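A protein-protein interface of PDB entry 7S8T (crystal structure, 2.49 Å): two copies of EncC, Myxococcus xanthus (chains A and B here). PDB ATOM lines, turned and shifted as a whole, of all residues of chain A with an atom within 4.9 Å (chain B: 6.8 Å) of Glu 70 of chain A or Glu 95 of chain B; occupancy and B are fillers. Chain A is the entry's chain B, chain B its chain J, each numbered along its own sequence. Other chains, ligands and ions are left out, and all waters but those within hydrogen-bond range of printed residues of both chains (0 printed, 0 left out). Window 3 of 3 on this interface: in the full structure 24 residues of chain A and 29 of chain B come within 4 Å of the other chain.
The side-chain carboxylate (OE1) of Glu 92 of chain B lies close to the backbone carbonyl oxygen (O) of Ala 73 of chain A (2.6 Å).
Among the printed residues, pairs that only touch across the chains: Ala 73 of chain A with His 89 of chain B, Ala 73 of chain A with Ala 88 of chain B, Leu 74 of chain A with Lys 96 of chain B, Glu 70 of chain A with Glu 95 of chain B and Leu 74 of chain A with Glu 92 of chain B.
A ring nitrogen (NE2) of His 89 of chain B sits close to the side-chain carboxylate (OE2) of Glu 92 of chain B (3.0 Å).
No position is printed for both chains.
Of the printed residues of chain B, Glu 70 of chain A touches Glu 95 (3.8 Å).
Of the printed residues of chain A, Ala 88 of chain B touches Ala 73 (3.2 Å).
Lys 91 of chain B touches none of the printed residues of chain A.
Val 94 of chain B touches none of the printed residues of chain A.
Glu 95 of chain B touches one residue of chain A.
Of the printed residues of chain A, Lys 96 of chain B touches Leu 74.
The nearest residue of chain B that does not touch Glu 70 of chain A is Ala 88 of chain B (4.1 Å).
Of the 11 printed residues of chain B, 5 touch a printed residue of chain A.
Hydrophobic or aromatic side chains of chain A within 4 Å of the printed part of chain B: Ala 73 and Leu 74.
Among the printed residues, 6 pairs touch across the chains.
Among the printed residues, no Asp or Glu carboxylate lies within 4 Å of a Lys or Arg side-chain nitrogen of the other chain.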
ATOM      1  N   ASP A  66      33.450 -25.608 -21.535  1.00  0.00           N
ATOM      2  CA  ASP A  66      33.469 -25.608 -20.075  1.00  0.00           C
ATOM      3  C   ASP A  66      32.152 -26.102 -19.504  1.00  0.00           C
ATOM      4  O   ASP A  66      32.131 -26.824 -18.504  1.00  0.00           O
ATOM      5  CB  ASP A  66      33.768 -24.197 -19.565  1.00  0.00           C
ATOM      6  CG  ASP A  66      33.649 -24.077 -18.050  1.00  0.00           C
ATOM      7  OD1 ASP A  66      34.507 -24.603 -17.307  1.00  0.00           O
ATOM      8  OD2 ASP A  66      32.685 -23.409 -17.611  1.00  0.00           O
ATOM      9  N   GLU A  67      31.043 -25.711 -20.115  1.00  0.00           N
ATOM     10  CA  GLU A  67      29.755 -26.191 -19.634  1.00  0.00           C
ATOM     11  C   GLU A  67      29.607 -27.691 -19.867  1.00  0.00           C
ATOM     12  O   GLU A  67      29.046 -28.400 -19.026  1.00  0.00           O
ATOM     13  CB  GLU A  67      28.626 -25.398 -20.284  1.00  0.00           C
ATOM     14  CG  GLU A  67      28.272 -24.161 -19.475  1.00  0.00           C
ATOM     15  CD  GLU A  67      27.122 -23.380 -20.062  1.00  0.00           C
ATOM     16  OE1 GLU A  67      26.644 -23.765 -21.141  1.00  0.00           O
ATOM     17  OE2 GLU A  67      26.694 -22.385 -19.441  1.00  0.00           O
ATOM     18  N   GLU A  68      30.132 -28.183 -20.993  1.00  0.00           N
ATOM     19  CA  GLU A  68      30.100 -29.653 -21.226  1.00  0.00           C
ATOM     20  C   GLU A  68      30.994 -30.329 -20.180  1.00  0.00           C
ATOM     21  O   GLU A  68      30.609 -31.408 -19.692  1.00  0.00           O
ATOM     22  CB  GLU A  68      30.525 -29.996 -22.656  1.00  0.00           C
ATOM     23  CG  GLU A  68      29.878 -29.124 -23.718  1.00  0.00           C
ATOM     24  CD  GLU A  68      28.402 -29.366 -23.993  1.00  0.00           C
ATOM     25  OE1 GLU A  68      27.710 -29.896 -23.104  1.00  0.00           O
ATOM     26  OE2 GLU A  68      27.947 -29.017 -25.100  1.00  0.00           O
ATOM     27  N   ARG A  69      32.136 -29.718 -19.845  1.00  0.00           N
ATOM     28  CA  ARG A  69      32.995 -30.271 -18.800  1.00  0.00           C
ATOM     29  C   ARG A  69      32.260 -30.309 -17.465  1.00  0.00           C
ATOM     30  O   ARG A  69      32.402 -31.262 -16.690  1.00  0.00           O
ATOM     31  CB  ARG A  69      34.286 -29.457 -18.689  1.00  0.00           C
ATOM     32  CG  ARG A  69      35.482 -30.250 -18.179  1.00  0.00           C
ATOM     33  CD  ARG A  69      36.784 -29.479 -18.354  1.00  0.00           C
ATOM     34  NE  ARG A  69      37.067 -29.171 -19.751  1.00  0.00           N
ATOM     35  CZ  ARG A  69      36.950 -27.960 -20.284  1.00  0.00           C
ATOM     36  NH1 ARG A  69      37.233 -27.764 -21.562  1.00  0.00           N
ATOM     37  NH2 ARG A  69      36.553 -26.942 -19.534  1.00  0.00           N
ATOM     38  N   GLU A  70      31.476 -29.268 -17.181  1.00  0.00           N
ATOM     39  CA  GLU A  70      30.629 -29.263 -15.994  1.00  0.00           C
ATOM     40  C   GLU A  70      29.639 -30.419 -16.037  1.00  0.00           C
ATOM     41  O   GLU A  70      29.422 -31.104 -15.030  1.00  0.00           O
ATOM     42  CB  GLU A  70      29.907 -27.916 -15.896  1.00  0.00           C
ATOM     43  CG  GLU A  70      28.940 -27.762 -14.737  1.00  0.00           C
ATOM     44  CD  GLU A  70      28.515 -26.316 -14.534  1.00  0.00           C
ATOM     45  OE1 GLU A  70      29.076 -25.432 -15.217  1.00  0.00           O
ATOM     46  OE2 GLU A  70      27.621 -26.065 -13.700  1.00  0.00           O
ATOM     47  N   HIS A  71      29.058 -30.659 -17.214  1.00  0.00           N
ATOM     48  CA  HIS A  71      28.126 -31.810 -17.359  1.00  0.00           C
ATOM     49  C   HIS A  71      28.879 -33.111 -17.069  1.00  0.00           C
ATOM     50  O   HIS A  71      28.329 -33.957 -16.336  1.00  0.00           O
ATOM     51  CB  HIS A  71      27.485 -31.820 -18.752  1.00  0.00           C
ATOM     52  CG  HIS A  71      26.961 -30.492 -19.180  1.00  0.00           C
ATOM     53  ND1 HIS A  71      26.967 -30.086 -20.498  1.00  0.00           N
ATOM     54  CD2 HIS A  71      26.419 -29.475 -18.478  1.00  0.00           C
ATOM     55  CE1 HIS A  71      26.450 -28.880 -20.592  1.00  0.00           C
ATOM     56  NE2 HIS A  71      26.112 -28.481 -19.369  1.00  0.00           N
ATOM     57  N   ALA A  72      30.091 -33.260 -17.616  1.00  0.00           N
ATOM     58  CA  ALA A  72      30.831 -34.503 -17.433  1.00  0.00           C
ATOM     59  C   ALA A  72      31.163 -34.728 -15.967  1.00  0.00           C
ATOM     60  O   ALA A  72      31.029 -35.846 -15.454  1.00  0.00           O
ATOM     61  CB  ALA A  72      32.108 -34.483 -18.276  1.00  0.00           C
ATOM     62  N   ALA A  73      31.563 -33.666 -15.269  1.00  0.00           N
ATOM     63  CA  ALA A  73      31.842 -33.782 -13.843  1.00  0.00           C
ATOM     64  C   ALA A  73      30.592 -34.175 -13.069  1.00  0.00           C
ATOM     65  O   ALA A  73      30.640 -35.039 -12.180  1.00  0.00           O
ATOM     66  CB  ALA A  73      32.401 -32.459 -13.321  1.00  0.00           C
ATOM     67  N   LEU A  74      29.453 -33.578 -13.420  1.00  0.00           N
ATOM     68  CA  LEU A  74      28.211 -33.881 -12.721  1.00  0.00           C
ATOM     69  C   LEU A  74      27.788 -35.327 -12.944  1.00  0.00           C
ATOM     70  O   LEU A  74      27.408 -36.030 -11.998  1.00  0.00           O
ATOM     71  CB  LEU A  74      27.117 -32.921 -13.179  1.00  0.00           C
ATOM     72  CG  LEU A  74      25.863 -32.926 -12.309  1.00  0.00           C
ATOM     73  CD1 LEU A  74      26.251 -32.859 -10.844  1.00  0.00           C
ATOM     74  CD2 LEU A  74      24.958 -31.769 -12.682  1.00  0.00           C
ATOM     75  N   ALA B  88      35.935 -27.615 -12.639  1.00  0.00           N
ATOM     76  CA  ALA B  88      34.592 -28.086 -12.945  1.00  0.00           C
ATOM     77  C   ALA B  88      34.343 -29.427 -12.272  1.00  0.00           C
ATOM     78  O   ALA B  88      33.223 -29.703 -11.829  1.00  0.00           O
ATOM     79  CB  ALA B  88      34.395 -28.189 -14.457  1.00  0.00           C
ATOM     80  N   HIS B  89      35.367 -30.275 -12.196  1.00  0.00           N
ATOM     81  CA  HIS B  89      35.270 -31.510 -11.434  1.00  0.00           C
ATOM     82  C   HIS B  89      35.643 -31.312  -9.970  1.00  0.00           C
ATOM     83  O   HIS B  89      35.843 -32.294  -9.247  1.00  0.00           O
ATOM     84  CB  HIS B  89      36.127 -32.608 -12.060  1.00  0.00           C
ATOM     85  CG  HIS B  89      35.628 -33.981 -11.749  1.00  0.00           C
ATOM     86  ND1 HIS B  89      34.596 -34.568 -12.447  1.00  0.00           N
ATOM     87  CD2 HIS B  89      36.003 -34.877 -10.807  1.00  0.00           C
ATOM     88  CE1 HIS B  89      34.346 -35.761 -11.941  1.00  0.00           C
ATOM     89  NE2 HIS B  89      35.193 -35.978 -10.951  1.00  0.00           N
ATOM     90  N   LYS B  91      33.776 -28.402  -8.577  1.00  0.00           N
ATOM     91  CA  LYS B  91      32.513 -27.734  -8.298  1.00  0.00           C
ATOM     92  C   LYS B  91      31.332 -28.651  -8.592  1.00  0.00           C
ATOM     93  O   LYS B  91      30.190 -28.188  -8.692  1.00  0.00           O
ATOM     94  CB  LYS B  91      32.417 -26.442  -9.113  1.00  0.00           C
ATOM     95  CG  LYS B  91      31.493 -25.379  -8.538  1.00  0.00           C
ATOM     96  CD  LYS B  91      32.056 -24.788  -7.259  1.00  0.00           C
ATOM     97  CE  LYS B  91      31.250 -23.582  -6.810  1.00  0.00           C
ATOM     98  NZ  LYS B  91      29.788 -23.807  -6.974  1.00  0.00           N
ATOM     99  N   GLU B  92      31.602 -29.950  -8.736  1.00  0.00           N
ATOM    100  CA  GLU B  92      30.587 -30.936  -9.081  1.00  0.00           C
ATOM    101  C   GLU B  92      29.806 -31.407  -7.859  1.00  0.00           C
ATOM    102  O   GLU B  92      28.589 -31.613  -7.939  1.00  0.00           O
ATOM    103  CB  GLU B  92      31.268 -32.132  -9.746  1.00  0.00           C
ATOM    104  CG  GLU B  92      32.444 -32.641  -8.908  1.00  0.00           C
ATOM    105  CD  GLU B  92      32.930 -34.016  -9.297  1.00  0.00           C
ATOM    106  OE1 GLU B  92      32.271 -34.672 -10.124  1.00  0.00           O
ATOM    107  OE2 GLU B  92      33.959 -34.456  -8.742  1.00  0.00           O
ATOM    108  N   ALA B  93      30.485 -31.582  -6.722  1.00  0.00           N
ATOM    109  CA  ALA B  93      29.807 -32.000  -5.501  1.00  0.00           C
ATOM    110  C   ALA B  93      28.887 -30.922  -4.953  1.00  0.00           C
ATOM    111  O   ALA B  93      27.930 -31.242  -4.241  1.00  0.00           O
ATOM    112  CB  ALA B  93      30.831 -32.401  -4.440  1.00  0.00           C
ATOM    113  N   VAL B  94      29.149 -29.660  -5.277  1.00  0.00           N
ATOM    114  CA  VAL B  94      28.277 -28.581  -4.839  1.00  0.00           C
ATOM    115  C   VAL B  94      27.131 -28.386  -5.824  1.00  0.00           C
ATOM    116  O   VAL B  94      26.024 -28.023  -5.420  1.00  0.00           O
ATOM    117  CB  VAL B  94      29.090 -27.285  -4.662  1.00  0.00           C
ATOM    118  CG1 VAL B  94      28.209 -26.151  -4.159  1.00  0.00           C
ATOM    119  CG2 VAL B  94      30.263 -27.522  -3.722  1.00  0.00           C
ATOM    120  N   GLU B  95      27.370 -28.664  -7.105  1.00  0.00           N
ATOM    121  CA  GLU B  95      26.346 -28.534  -8.131  1.00  0.00           C
ATOM    122  C   GLU B  95      25.400 -29.730  -8.178  1.00  0.00           C
ATOM    123  O   GLU B  95      24.290 -29.607  -8.707  1.00  0.00           O
ATOM    124  CB  GLU B  95      27.014 -28.324  -9.497  1.00  0.00           C
ATOM    125  CG  GLU B  95      26.077 -28.327 -10.698  1.00  0.00           C
ATOM    126  CD  GLU B  95      25.191 -27.095 -10.759  1.00  0.00           C
ATOM    127  OE1 GLU B  95      25.203 -26.287  -9.809  1.00  0.00           O
ATOM    128  OE2 GLU B  95      24.470 -26.935 -11.761  1.00  0.00           O
ATOM    129  N   LYS B  96      25.792 -30.870  -7.607  1.00  0.00           N
ATOM    130  CA  LYS B  96      24.885 -32.012  -7.559  1.00  0.00           C
ATOM    131  C   LYS B  96      23.678 -31.747  -6.664  1.00  0.00           C
ATOM    132  O   LYS B  96      22.529 -31.855  -7.106  1.00  0.00           O
ATOM    133  CB  LYS B  96      25.654 -33.237  -7.065  1.00  0.00           C
ATOM    134  CG  LYS B  96      24.839 -34.496  -6.985  1.00  0.00           C
ATOM    135  CD  LYS B  96      24.289 -34.863  -8.339  1.00  0.00           C
ATOM    136  CE  LYS B  96      23.625 -36.210  -8.279  1.00  0.00           C
ATOM    137  NZ  LYS B  96      24.645 -37.251  -8.022  1.00  0.00           N
ATOM    138  N   TYR B  97      23.920 -31.382  -5.406  1.00  0.00           N
ATOM    139  CA  TYR B  97      22.837 -31.083  -4.474  1.00  0.00           C
ATOM    140  C   TYR B  97      22.143 -29.767  -4.795  1.00  0.00           C
ATOM    141  O   TYR B  97      21.012 -29.547  -4.349  1.00  0.00           O
ATOM    142  CB  TYR B  97      23.364 -31.064  -3.039  1.00  0.00           C
ATOM    143  N   ARG B  98      22.795 -28.899  -5.569  1.00  0.00           N
ATOM    144  CA  ARG B  98      22.379 -27.536  -5.879  1.00  0.00           C
ATOM    145  C   ARG B  98      21.103 -27.454  -6.710  1.00  0.00           C
ATOM    146  O   ARG B  98      20.642 -26.339  -6.982  1.00  0.00           O
ATOM    147  CB  ARG B  98      23.523 -26.822  -6.605  1.00  0.00           C
ATOM    148  CG  ARG B  98      23.436 -25.310  -6.644  1.00  0.00           C
ATOM    149  CD  ARG B  98      23.092 -24.738  -5.285  1.00  0.00           C
ATOM    150  NE  ARG B  98      22.805 -23.310  -5.368  1.00  0.00           N
ATOM    151  CZ  ARG B  98      21.672 -22.807  -5.849  1.00  0.00           C
ATOM    152  NH1 ARG B  98      20.717 -23.614  -6.290  1.00  0.00           N
ATOM    153  NH2 ARG B  98      21.494 -21.493  -5.889  1.00  0.00           N
ATOM    154  N   LEU B  99      20.489 -28.572  -7.078  1.00  0.00           N
ATOM    155  CA  LEU B  99      19.246 -28.551  -7.847  1.00  0.00           C
ATOM    156  C   LEU B  99      18.088 -28.746  -6.874  1.00  0.00           C
ATOM    157  O   LEU B  99      17.615 -29.862  -6.653  1.00  0.00           O
ATOM    158  CB  LEU B  99      19.253 -29.631  -8.922  1.00  0.00           C
ATOM    159  CG  LEU B  99      19.738 -29.252 -10.317  1.00  0.00           C
ATOM    160  CD1 LEU B  99      19.474 -30.401 -11.259  1.00  0.00           C
ATOM    161  CD2 LEU B  99      19.046 -27.990 -10.800  1.00  0.00           C
